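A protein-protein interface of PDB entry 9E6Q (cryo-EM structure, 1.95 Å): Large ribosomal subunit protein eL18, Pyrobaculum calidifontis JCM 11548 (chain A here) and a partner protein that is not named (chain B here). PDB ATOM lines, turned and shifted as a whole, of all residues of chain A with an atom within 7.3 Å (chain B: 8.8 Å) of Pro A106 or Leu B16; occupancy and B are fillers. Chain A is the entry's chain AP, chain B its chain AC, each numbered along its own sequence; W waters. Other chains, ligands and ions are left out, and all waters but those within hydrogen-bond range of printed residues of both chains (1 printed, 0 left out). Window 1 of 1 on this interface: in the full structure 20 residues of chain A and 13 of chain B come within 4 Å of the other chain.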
ATOM      1  N   ARG A  11     -21.978  22.474   6.984  1.00  0.00           N
ATOM      2  CA  ARG A  11     -20.755  22.457   6.191  1.00  0.00           C
ATOM      3  C   ARG A  11     -20.270  21.043   5.924  1.00  0.00           C
ATOM      4  O   ARG A  11     -19.617  20.799   4.908  1.00  0.00           O
ATOM      5  CB  ARG A  11     -19.657  23.249   6.890  1.00  0.00           C
ATOM      6  CG  ARG A  11     -19.627  24.705   6.539  1.00  0.00           C
ATOM      7  CD  ARG A  11     -18.903  25.488   7.600  1.00  0.00           C
ATOM      8  NE  ARG A  11     -18.783  26.895   7.248  1.00  0.00           N
ATOM      9  CZ  ARG A  11     -17.984  27.748   7.871  1.00  0.00           C
ATOM     10  NH1 ARG A  11     -17.201  27.362   8.863  1.00  0.00           N
ATOM     11  NH2 ARG A  11     -17.968  29.020   7.486  1.00  0.00           N
ATOM     12  N   GLN A  12     -20.551  20.108   6.830  1.00  0.00           N
ATOM     13  CA  GLN A  12     -20.198  18.716   6.583  1.00  0.00           C
ATOM     14  C   GLN A  12     -20.893  18.206   5.334  1.00  0.00           C
ATOM     15  O   GLN A  12     -20.291  17.521   4.503  1.00  0.00           O
ATOM     16  CB  GLN A  12     -20.575  17.855   7.787  1.00  0.00           C
ATOM     17  CG  GLN A  12     -20.006  18.331   9.108  1.00  0.00           C
ATOM     18  CD  GLN A  12     -18.501  18.427   9.088  1.00  0.00           C
ATOM     19  OE1 GLN A  12     -17.818  17.502   8.658  1.00  0.00           O
ATOM     20  NE2 GLN A  12     -17.972  19.549   9.556  1.00  0.00           N
ATOM     21  N   ARG A  14     -22.031  20.215   2.945  1.00  0.00           N
ATOM     22  CA  ARG A  14     -21.511  21.002   1.831  1.00  0.00           C
ATOM     23  C   ARG A  14     -20.178  20.459   1.342  1.00  0.00           C
ATOM     24  O   ARG A  14     -19.923  20.414   0.136  1.00  0.00           O
ATOM     25  CB  ARG A  14     -21.375  22.471   2.235  1.00  0.00           C
ATOM     26  CG  ARG A  14     -22.690  23.200   2.391  1.00  0.00           C
ATOM     27  CD  ARG A  14     -22.484  24.643   2.801  1.00  0.00           C
ATOM     28  NE  ARG A  14     -22.253  25.517   1.658  1.00  0.00           N
ATOM     29  CZ  ARG A  14     -23.199  26.184   1.014  1.00  0.00           C
ATOM     30  NH1 ARG A  14     -24.468  26.107   1.374  1.00  0.00           N
ATOM     31  NH2 ARG A  14     -22.864  26.945  -0.020  1.00  0.00           N
ATOM     32  N   MET A  15     -19.307  20.054   2.263  1.00  0.00           N
ATOM     33  CA  MET A  15     -18.015  19.519   1.859  1.00  0.00           C
ATOM     34  C   MET A  15     -18.164  18.161   1.189  1.00  0.00           C
ATOM     35  O   MET A  15     -17.411  17.834   0.268  1.00  0.00           O
ATOM     36  CB  MET A  15     -17.088  19.429   3.063  1.00  0.00           C
ATOM     37  CG  MET A  15     -16.471  20.750   3.470  1.00  0.00           C
ATOM     38  SD  MET A  15     -16.552  22.022   2.197  1.00  0.00           S
ATOM     39  CE  MET A  15     -15.064  21.673   1.280  1.00  0.00           C
ATOM     40  N   LEU A  16     -19.126  17.355   1.640  1.00  0.00           N
ATOM     41  CA  LEU A  16     -19.373  16.065   1.007  1.00  0.00           C
ATOM     42  C   LEU A  16     -19.851  16.235  -0.426  1.00  0.00           C
ATOM     43  O   LEU A  16     -19.457  15.474  -1.313  1.00  0.00           O
ATOM     44  CB  LEU A  16     -20.396  15.270   1.813  1.00  0.00           C
ATOM     45  CG  LEU A  16     -20.844  13.967   1.155  1.00  0.00           C
ATOM     46  CD1 LEU A  16     -19.672  13.017   1.021  1.00  0.00           C
ATOM     47  CD2 LEU A  16     -21.969  13.332   1.932  1.00  0.00           C
ATOM     48  N   ILE A  17     -20.709  17.223  -0.670  1.00  0.00           N
ATOM     49  CA  ILE A  17     -21.195  17.476  -2.020  1.00  0.00           C
ATOM     50  C   ILE A  17     -20.053  17.914  -2.925  1.00  0.00           C
ATOM     51  O   ILE A  17     -19.965  17.494  -4.081  1.00  0.00           O
ATOM     52  CB  ILE A  17     -22.337  18.509  -1.984  1.00  0.00           C
ATOM     53  CG1 ILE A  17     -23.613  17.861  -1.445  1.00  0.00           C
ATOM     54  CG2 ILE A  17     -22.576  19.093  -3.348  1.00  0.00           C
ATOM     55  CD1 ILE A  17     -24.612  18.833  -0.880  1.00  0.00           C
ATOM     56  N   ARG A  18     -19.154  18.758  -2.413  1.00  0.00           N
ATOM     57  CA  ARG A  18     -17.982  19.146  -3.190  1.00  0.00           C
ATOM     58  C   ARG A  18     -17.094  17.947  -3.485  1.00  0.00           C
ATOM     59  O   ARG A  18     -16.590  17.799  -4.602  1.00  0.00           O
ATOM     60  CB  ARG A  18     -17.197  20.228  -2.452  1.00  0.00           C
ATOM     61  CG  ARG A  18     -15.878  20.591  -3.092  1.00  0.00           C
ATOM     62  CD  ARG A  18     -16.078  21.385  -4.363  1.00  0.00           C
ATOM     63  NE  ARG A  18     -14.808  21.806  -4.942  1.00  0.00           N
ATOM     64  CZ  ARG A  18     -14.611  22.045  -6.231  1.00  0.00           C
ATOM     65  NH1 ARG A  18     -15.591  21.937  -7.111  1.00  0.00           N
ATOM     66  NH2 ARG A  18     -13.400  22.392  -6.648  1.00  0.00           N
ATOM     67  N   PHE A  19     -16.901  17.073  -2.496  1.00  0.00           N
ATOM     68  CA  PHE A  19     -16.117  15.857  -2.688  1.00  0.00           C
ATOM     69  C   PHE A  19     -16.674  15.015  -3.829  1.00  0.00           C
ATOM     70  O   PHE A  19     -15.931  14.565  -4.705  1.00  0.00           O
ATOM     71  CB  PHE A  19     -16.109  15.058  -1.385  1.00  0.00           C
ATOM     72  CG  PHE A  19     -15.459  13.706  -1.483  1.00  0.00           C
ATOM     73  CD1 PHE A  19     -16.183  12.595  -1.876  1.00  0.00           C
ATOM     74  CD2 PHE A  19     -14.140  13.538  -1.127  1.00  0.00           C
ATOM     75  CE1 PHE A  19     -15.592  11.361  -1.947  1.00  0.00           C
ATOM     76  CE2 PHE A  19     -13.549  12.301  -1.189  1.00  0.00           C
ATOM     77  CZ  PHE A  19     -14.273  11.213  -1.601  1.00  0.00           C
ATOM     78  N   LEU A  20     -17.987  14.793  -3.830  1.00  0.00           N
ATOM     79  CA  LEU A  20     -18.594  13.924  -4.829  1.00  0.00           C
ATOM     80  C   LEU A  20     -18.460  14.505  -6.226  1.00  0.00           C
ATOM     81  O   LEU A  20     -18.270  13.766  -7.195  1.00  0.00           O
ATOM     82  CB  LEU A  20     -20.058  13.679  -4.482  1.00  0.00           C
ATOM     83  CG  LEU A  20     -20.272  12.741  -3.298  1.00  0.00           C
ATOM     84  CD1 LEU A  20     -21.669  12.885  -2.742  1.00  0.00           C
ATOM     85  CD2 LEU A  20     -20.003  11.316  -3.712  1.00  0.00           C
ATOM     86  N   ALA A  83     -23.335   2.188   1.772  1.00  0.00           N
ATOM     87  CA  ALA A  83     -22.807   3.492   2.130  1.00  0.00           C
ATOM     88  C   ALA A  83     -23.937   4.510   2.095  1.00  0.00           C
ATOM     89  O   ALA A  83     -24.839   4.425   1.261  1.00  0.00           O
ATOM     90  CB  ALA A  83     -21.690   3.919   1.181  1.00  0.00           C
ATOM     91  N   ALA A  84     -23.890   5.468   3.011  1.00  0.00           N
ATOM     92  CA  ALA A  84     -24.957   6.450   3.125  1.00  0.00           C
ATOM     93  C   ALA A  84     -24.396   7.715   3.749  1.00  0.00           C
ATOM     94  O   ALA A  84     -23.298   7.721   4.305  1.00  0.00           O
ATOM     95  CB  ALA A  84     -26.125   5.910   3.951  1.00  0.00           C
ATOM     96  N   VAL A  85     -25.170   8.797   3.640  1.00  0.00           N
ATOM     97  CA  VAL A  85     -24.785  10.048   4.286  1.00  0.00           C
ATOM     98  C   VAL A  85     -24.748   9.873   5.797  1.00  0.00           C
ATOM     99  O   VAL A  85     -23.813  10.327   6.464  1.00  0.00           O
ATOM    100  CB  VAL A  85     -25.735  11.184   3.866  1.00  0.00           C
ATOM    101  CG1 VAL A  85     -25.459  12.433   4.672  1.00  0.00           C
ATOM    102  CG2 VAL A  85     -25.604  11.467   2.381  1.00  0.00           C
ATOM    103  N   LEU A 103     -20.552   1.697   5.358  1.00  0.00           N
ATOM    104  CA  LEU A 103     -19.479   2.594   4.971  1.00  0.00           C
ATOM    105  C   LEU A 103     -19.975   4.029   4.898  1.00  0.00           C
ATOM    106  O   LEU A 103     -21.173   4.296   4.807  1.00  0.00           O
ATOM    107  CB  LEU A 103     -18.886   2.218   3.613  1.00  0.00           C
ATOM    108  CG  LEU A 103     -18.494   0.771   3.371  1.00  0.00           C
ATOM    109  CD1 LEU A 103     -18.137   0.587   1.913  1.00  0.00           C
ATOM    110  CD2 LEU A 103     -17.341   0.400   4.263  1.00  0.00           C
ATOM    111  N   THR A 104     -19.029   4.956   4.950  1.00  0.00           N
ATOM    112  CA  THR A 104     -19.305   6.309   4.515  1.00  0.00           C
ATOM    113  C   THR A 104     -19.168   6.390   3.002  1.00  0.00           C
ATOM    114  O   THR A 104     -18.498   5.574   2.370  1.00  0.00           O
ATOM    115  CB  THR A 104     -18.362   7.308   5.183  1.00  0.00           C
ATOM    116  OG1 THR A 104     -17.027   7.085   4.722  1.00  0.00           O
ATOM    117  CG2 THR A 104     -18.401   7.152   6.678  1.00  0.00           C
ATOM    118  N   ILE A 105     -19.836   7.381   2.419  1.00  0.00           N
ATOM    119  CA  ILE A 105     -19.734   7.588   0.974  1.00  0.00           C
ATOM    120  C   ILE A 105     -18.299   7.850   0.540  1.00  0.00           C
ATOM    121  O   ILE A 105     -17.880   7.296  -0.483  1.00  0.00           O
ATOM    122  CB  ILE A 105     -20.722   8.672   0.527  1.00  0.00           C
ATOM    123  CG1 ILE A 105     -22.152   8.170   0.719  1.00  0.00           C
ATOM    124  CG2 ILE A 105     -20.490   9.042  -0.910  1.00  0.00           C
ATOM    125  CD1 ILE A 105     -23.196   9.220   0.546  1.00  0.00           C
ATOM    126  N   PRO A 106     -17.497   8.667   1.235  1.00  0.00           N
ATOM    127  CA  PRO A 106     -16.080   8.777   0.850  1.00  0.00           C
ATOM    128  C   PRO A 106     -15.311   7.471   0.941  1.00  0.00           C
ATOM    129  O   PRO A 106     -14.399   7.253   0.139  1.00  0.00           O
ATOM    130  CB  PRO A 106     -15.535   9.822   1.828  1.00  0.00           C
ATOM    131  CG  PRO A 106     -16.703  10.619   2.203  1.00  0.00           C
ATOM    132  CD  PRO A 106     -17.847   9.670   2.255  1.00  0.00           C
ATOM    133  N   GLU A 107     -15.638   6.603   1.896  1.00  0.00           N
ATOM    134  CA  GLU A 107     -14.997   5.292   1.956  1.00  0.00           C
ATOM    135  C   GLU A 107     -15.309   4.475   0.713  1.00  0.00           C
ATOM    136  O   GLU A 107     -14.430   3.812   0.156  1.00  0.00           O
ATOM    137  CB  GLU A 107     -15.452   4.540   3.199  1.00  0.00           C
ATOM    138  CG  GLU A 107     -14.509   4.618   4.363  1.00  0.00           C
ATOM    139  CD  GLU A 107     -15.242   4.713   5.674  1.00  0.00           C
ATOM    140  OE1 GLU A 107     -16.154   3.893   5.898  1.00  0.00           O
ATOM    141  OE2 GLU A 107     -14.908   5.610   6.477  1.00  0.00           O
ATOM    142  N   LEU A 108     -16.568   4.491   0.279  1.00  0.00           N
ATOM    143  CA  LEU A 108     -16.949   3.748  -0.914  1.00  0.00           C
ATOM    144  C   LEU A 108     -16.253   4.292  -2.150  1.00  0.00           C
ATOM    145  O   LEU A 108     -15.812   3.524  -3.010  1.00  0.00           O
ATOM    146  CB  LEU A 108     -18.463   3.789  -1.094  1.00  0.00           C
ATOM    147  CG  LEU A 108     -19.005   3.137  -2.364  1.00  0.00           C
ATOM    148  CD1 LEU A 108     -18.619   1.679  -2.416  1.00  0.00           C
ATOM    149  CD2 LEU A 108     -20.508   3.294  -2.433  1.00  0.00           C
ATOM    150  N   VAL A 109     -16.148   5.615  -2.259  1.00  0.00           N
ATOM    151  CA  VAL A 109     -15.494   6.213  -3.418  1.00  0.00           C
ATOM    152  C   VAL A 109     -14.016   5.852  -3.442  1.00  0.00           C
ATOM    153  O   VAL A 109     -13.461   5.532  -4.496  1.00  0.00           O
ATOM    154  CB  VAL A 109     -15.712   7.736  -3.431  1.00  0.00           C
ATOM    155  CG1 VAL A 109     -14.844   8.386  -4.485  1.00  0.00           C
ATOM    156  CG2 VAL A 109     -17.169   8.055  -3.675  1.00  0.00           C
ATOM    157  N   ARG A 110     -13.352   5.902  -2.289  1.00  0.00           N
ATOM    158  CA  ARG A 110     -11.949   5.505  -2.241  1.00  0.00           C
ATOM    159  C   ARG A 110     -11.784   4.036  -2.602  1.00  0.00           C
ATOM    160  O   ARG A 110     -10.864   3.667  -3.338  1.00  0.00           O
ATOM    161  CB  ARG A 110     -11.365   5.784  -0.858  1.00  0.00           C
ATOM    162  CG  ARG A 110     -11.205   7.255  -0.534  1.00  0.00           C
ATOM    163  CD  ARG A 110     -10.368   7.458   0.714  1.00  0.00           C
ATOM    164  NE  ARG A 110     -11.140   7.249   1.932  1.00  0.00           N
ATOM    165  CZ  ARG A 110     -11.858   8.184   2.537  1.00  0.00           C
ATOM    166  NH1 ARG A 110     -11.931   9.414   2.063  1.00  0.00           N
ATOM    167  NH2 ARG A 110     -12.522   7.876   3.643  1.00  0.00           N
ATOM    168  N   ARG A 111     -12.668   3.181  -2.088  1.00  0.00           N
ATOM    169  CA  ARG A 111     -12.605   1.759  -2.402  1.00  0.00           C
ATOM    170  C   ARG A 111     -12.928   1.494  -3.866  1.00  0.00           C
ATOM    171  O   ARG A 111     -12.315   0.628  -4.499  1.00  0.00           O
ATOM    172  CB  ARG A 111     -13.560   0.994  -1.489  1.00  0.00           C
ATOM    173  CG  ARG A 111     -13.858  -0.416  -1.927  1.00  0.00           C
ATOM    174  CD  ARG A 111     -14.854  -1.076  -0.997  1.00  0.00           C
ATOM    175  NE  ARG A 111     -14.402  -1.044   0.386  1.00  0.00           N
ATOM    176  CZ  ARG A 111     -15.001  -1.674   1.387  1.00  0.00           C
ATOM    177  NH1 ARG A 111     -16.081  -2.409   1.192  1.00  0.00           N
ATOM    178  NH2 ARG A 111     -14.499  -1.569   2.611  1.00  0.00           N
ATOM    179  N   ASN A 112     -13.894   2.218  -4.419  1.00  0.00           N
ATOM    180  CA  ASN A 112     -14.386   1.978  -5.775  1.00  0.00           C
ATOM    181  C   ASN A 112     -14.505   3.303  -6.512  1.00  0.00           C
ATOM    182  O   ASN A 112     -15.601   3.855  -6.657  1.00  0.00           O
ATOM    183  CB  ASN A 112     -15.728   1.249  -5.736  1.00  0.00           C
ATOM    184  CG  ASN A 112     -16.087   0.618  -7.051  1.00  0.00           C
ATOM    185  OD1 ASN A 112     -15.527   0.954  -8.090  1.00  0.00           O
ATOM    186  ND2 ASN A 112     -17.034  -0.304  -7.018  1.00  0.00           N
ATOM    187  N   LYS B  10     -16.779   7.177  12.519  1.00  0.00           N
ATOM    188  CA  LYS B  10     -16.312   7.497  11.176  1.00  0.00           C
ATOM    189  C   LYS B  10     -17.210   8.526  10.503  1.00  0.00           C
ATOM    190  O   LYS B  10     -16.740   9.295   9.660  1.00  0.00           O
ATOM    191  CB  LYS B  10     -16.228   6.227  10.334  1.00  0.00           C
ATOM    192  CG  LYS B  10     -17.576   5.646   9.963  1.00  0.00           C
ATOM    193  CD  LYS B  10     -17.590   4.145  10.078  1.00  0.00           C
ATOM    194  CE  LYS B  10     -17.295   3.495   8.758  1.00  0.00           C
ATOM    195  NZ  LYS B  10     -17.369   2.018   8.834  1.00  0.00           N
ATOM    196  N   PHE B  11     -18.493   8.560  10.859  1.00  0.00           N
ATOM    197  CA  PHE B  11     -19.402   9.543  10.287  1.00  0.00           C
ATOM    198  C   PHE B  11     -19.255  10.914  10.928  1.00  0.00           C
ATOM    199  O   PHE B  11     -19.729  11.899  10.357  1.00  0.00           O
ATOM    200  CB  PHE B  11     -20.849   9.072  10.421  1.00  0.00           C
ATOM    201  CG  PHE B  11     -21.237   8.006   9.442  1.00  0.00           C
ATOM    202  CD1 PHE B  11     -21.654   8.336   8.169  1.00  0.00           C
ATOM    203  CD2 PHE B  11     -21.190   6.674   9.797  1.00  0.00           C
ATOM    204  CE1 PHE B  11     -22.007   7.361   7.271  1.00  0.00           C
ATOM    205  CE2 PHE B  11     -21.546   5.695   8.901  1.00  0.00           C
ATOM    206  CZ  PHE B  11     -21.958   6.039   7.637  1.00  0.00           C
ATOM    207  N   LEU B  13     -16.017  12.430  12.218  1.00  0.00           N
ATOM    208  CA  LEU B  13     -14.819  12.963  11.582  1.00  0.00           C
ATOM    209  C   LEU B  13     -14.754  12.377  10.183  1.00  0.00           C
ATOM    210  O   LEU B  13     -14.160  11.325   9.953  1.00  0.00           O
ATOM    211  CB  LEU B  13     -13.579  12.621  12.394  1.00  0.00           C
ATOM    212  CG  LEU B  13     -13.672  12.910  13.893  1.00  0.00           C
ATOM    213  CD1 LEU B  13     -12.880  11.883  14.675  1.00  0.00           C
ATOM    214  CD2 LEU B  13     -13.201  14.328  14.216  1.00  0.00           C
ATOM    215  N   LEU B  14     -15.383  13.063   9.237  1.00  0.00           N
ATOM    216  CA  LEU B  14     -15.476  12.561   7.876  1.00  0.00           C
ATOM    217  C   LEU B  14     -14.175  12.804   7.125  1.00  0.00           C
ATOM    218  O   LEU B  14     -13.710  13.941   7.016  1.00  0.00           O
ATOM    219  CB  LEU B  14     -16.639  13.225   7.144  1.00  0.00           C
ATOM    220  CG  LEU B  14     -17.202  12.438   5.965  1.00  0.00           C
ATOM    221  CD1 LEU B  14     -17.631  11.062   6.421  1.00  0.00           C
ATOM    222  CD2 LEU B  14     -18.362  13.176   5.365  1.00  0.00           C
ATOM    223  N   ASP B  15     -13.596  11.729   6.605  1.00  0.00           N
ATOM    224  CA  ASP B  15     -12.367  11.786   5.828  1.00  0.00           C
ATOM    225  C   ASP B  15     -12.735  12.063   4.377  1.00  0.00           C
ATOM    226  O   ASP B  15     -13.425  11.260   3.747  1.00  0.00           O
ATOM    227  CB  ASP B  15     -11.612  10.464   5.968  1.00  0.00           C
ATOM    228  CG  ASP B  15     -10.298  10.436   5.207  1.00  0.00           C
ATOM    229  OD1 ASP B  15     -10.034  11.328   4.382  1.00  0.00           O
ATOM    230  OD2 ASP B  15      -9.524   9.485   5.428  1.00  0.00           O
ATOM    231  N   LEU B  16     -12.278  13.193   3.845  1.00  0.00           N
ATOM    232  CA  LEU B  16     -12.596  13.571   2.475  1.00  0.00           C
ATOM    233  C   LEU B  16     -11.391  13.474   1.550  1.00  0.00           C
ATOM    234  O   LEU B  16     -11.408  14.044   0.458  1.00  0.00           O
ATOM    235  CB  LEU B  16     -13.183  14.978   2.434  1.00  0.00           C
ATOM    236  CG  LEU B  16     -14.528  15.134   3.140  1.00  0.00           C
ATOM    237  CD1 LEU B  16     -14.957  16.578   3.112  1.00  0.00           C
ATOM    238  CD2 LEU B  16     -15.581  14.250   2.514  1.00  0.00           C
ATOM    239  N   SER B  17     -10.347  12.770   1.965  1.00  0.00           N
ATOM    240  CA  SER B  17      -9.218  12.538   1.088  1.00  0.00           C
ATOM    241  C   SER B  17      -9.616  11.567  -0.021  1.00  0.00           C
ATOM    242  O   SER B  17     -10.506  10.736   0.165  1.00  0.00           O
ATOM    243  CB  SER B  17      -8.038  11.984   1.879  1.00  0.00           C
ATOM    244  OG  SER B  17      -8.395  10.791   2.552  1.00  0.00           O
ATOM    245  N   PRO B  18      -8.972  11.646  -1.190  1.00  0.00           N
ATOM    246  CA  PRO B  18      -7.865  12.529  -1.565  1.00  0.00           C
ATOM    247  C   PRO B  18      -8.299  13.840  -2.205  1.00  0.00           C
ATOM    248  O   PRO B  18      -7.469  14.707  -2.436  1.00  0.00           O
ATOM    249  CB  PRO B  18      -7.101  11.667  -2.565  1.00  0.00           C
ATOM    250  CG  PRO B  18      -8.205  10.964  -3.310  1.00  0.00           C
ATOM    251  CD  PRO B  18      -9.291  10.708  -2.281  1.00  0.00           C
ATOM    252  N   TYR B  19      -9.585  14.023  -2.499  1.00  0.00           N
ATOM    253  CA  TYR B  19     -10.006  15.152  -3.319  1.00  0.00           C
ATOM    254  C   TYR B  19     -10.081  16.458  -2.547  1.00  0.00           C
ATOM    255  O   TYR B  19     -10.011  17.525  -3.161  1.00  0.00           O
ATOM    256  CB  TYR B  19     -11.349  14.840  -3.970  1.00  0.00           C
ATOM    257  CG  TYR B  19     -11.322  13.550  -4.740  1.00  0.00           C
ATOM    258  CD1 TYR B  19     -10.537  13.421  -5.870  1.00  0.00           C
ATOM    259  CD2 TYR B  19     -12.061  12.455  -4.328  1.00  0.00           C
ATOM    260  CE1 TYR B  19     -10.494  12.251  -6.567  1.00  0.00           C
ATOM    261  CE2 TYR B  19     -12.024  11.276  -5.028  1.00  0.00           C
ATOM    262  CZ  TYR B  19     -11.238  11.182  -6.148  1.00  0.00           C
ATOM    263  OH  TYR B  19     -11.192  10.013  -6.860  1.00  0.00           O
ATOM    264  N   ILE B  20     -10.223  16.412  -1.228  1.00  0.00           N
ATOM    265  CA  ILE B  20     -10.275  17.612  -0.406  1.00  0.00           C
ATOM    266  C   ILE B  20      -9.137  17.552   0.603  1.00  0.00           C
ATOM    267  O   ILE B  20      -8.993  16.560   1.324  1.00  0.00           O
ATOM    268  CB  ILE B  20     -11.636  17.759   0.293  1.00  0.00           C
ATOM    269  CG1 ILE B  20     -12.747  17.866  -0.753  1.00  0.00           C
ATOM    270  CG2 ILE B  20     -11.636  18.968   1.196  1.00  0.00           C
ATOM    271  CD1 ILE B  20     -14.078  18.254  -0.194  1.00  0.00           C
ATOM    272  N   LYS B  21      -8.334  18.610   0.644  1.00  0.00           N
ATOM    273  CA  LYS B  21      -7.152  18.623   1.492  1.00  0.00           C
ATOM    274  C   LYS B  21      -7.552  18.658   2.965  1.00  0.00           C
ATOM    275  O   LYS B  21      -8.531  19.312   3.329  1.00  0.00           O
ATOM    276  CB  LYS B  21      -6.278  19.828   1.159  1.00  0.00           C
ATOM    277  CG  LYS B  21      -7.014  20.925   0.413  1.00  0.00           C
ATOM    278  CD  LYS B  21      -6.218  22.214   0.400  1.00  0.00           C
ATOM    279  CE  LYS B  21      -5.175  22.214  -0.704  1.00  0.00           C
ATOM    280  NZ  LYS B  21      -4.506  23.536  -0.822  1.00  0.00           N
ATOM    281  N   PRO B  22      -6.814  17.974   3.832  1.00  0.00           N
ATOM    282  CA  PRO B  22      -7.213  17.891   5.239  1.00  0.00           C
ATOM    283  C   PRO B  22      -7.078  19.222   5.960  1.00  0.00           C
ATOM    284  O   PRO B  22      -6.258  20.072   5.603  1.00  0.00           O
ATOM    285  CB  PRO B  22      -6.238  16.857   5.814  1.00  0.00           C
ATOM    286  CG  PRO B  22      -5.735  16.114   4.613  1.00  0.00           C
ATOM    287  CD  PRO B  22      -5.610  17.176   3.577  1.00  0.00           C
ATOM    288  N   ALA B  23      -7.905  19.397   6.986  1.00  0.00           N
ATOM    289  CA  ALA B  23      -7.811  20.539   7.882  1.00  0.00           C
ATOM    290  C   ALA B  23      -6.959  20.161   9.095  1.00  0.00           C
ATOM    291  O   ALA B  23      -6.278  19.133   9.103  1.00  0.00           O
ATOM    292  CB  ALA B  23      -9.205  21.013   8.283  1.00  0.00           C
HETATM  293  O   HOH W   1     -15.089   8.919   5.363  1.00  0.00           O
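The guanidinium group (NH1) of Arg A110 is in hydrogen-bond range of the backbone carbonyl oxygen (O) of Ser B17 (2.7 Å). The side-chain carboxylate (OE1) of Glu A107 is in salt-bridge range of the side-chain amino group (NZ) of Lys B10, 3.7 Å away. The side-chain carboxylate (OD1) of Asp B15 lies within salt-bridge range of the guanidinium group (NH1) of Arg A110.
The side-chain hydroxyl (OG) of Ser B17 lies within hydrogen-bond range of the side-chain carboxylate (OD1) of Asp B15, at 2.5 Å. The backbone NH (N) of Ala A84 lies within hydrogen-bond range of the backbone carbonyl oxygen (O) of Leu A103. The side-chain carboxylate of Glu A107 lies close to the side-chain hydroxyl of Thr A104.
Leu B16 touches Met A15. Met A15 touches Ile B20 (O to CD1, 3.4 Å). Leu B16 touches Phe A19 (O to CD2, 3.2 Å). Phe A19 touches Ser B17. N of Phe A19 touches CD1 of Ile B20 (3.8 Å). Ala A84 touches Phe B11. Val A85 touches Phe B11 (O to CD1, 3.4 Å). Phe B11 touches Leu A103. Thr A104 touches Leu B14 (CG2 to CD1, 3.99 Å). O of Asp B15 touches CB of Pro A106 (3.2 Å).
Arg A11 touches none of the printed residues of chain B. Of the printed residues of chain B, Val A85 touches Phe B11. Pro A106 touches just these residues of chain B: Asp B15 (3.2 Å) and Leu B16 (3.8 Å). Printed residues of chain A within 4 Å of Asp B15: Pro A106 and Arg A110. The nearest residue of chain A that does not touch Leu B16 is Arg A110 (4.1 Å).
Hydrophobic or aromatic side chains of chain B within 4 Å of the printed part of chain A: Phe B11, Leu B14, Leu B16, Tyr B19 and Ile B20. Along chain B the printed residues that touch a printed residue of chain A span positions 10 to 20. Of the 22 printed residues of chain A, 9 touch a printed residue of chain B. Hydrophobic or aromatic side chains of chain A within 4 Å of the printed part of chain B: Met A15, Phe A19 and Pro A106. Among the printed residues, Asp or Glu carboxylates within 4 Å of a Lys or Arg side-chain nitrogen of the other chain: Glu A107 with Lys B10 and Arg A110 with Asp B15.
Water W1 lies within hydrogen-bond range of OG1 of Thr A104 (2.7 Å), NH2 of Arg A110 (3.3 Å), O of Asp B15 (3.3 Å) and OE2 of Glu A107 (3.5 Å).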
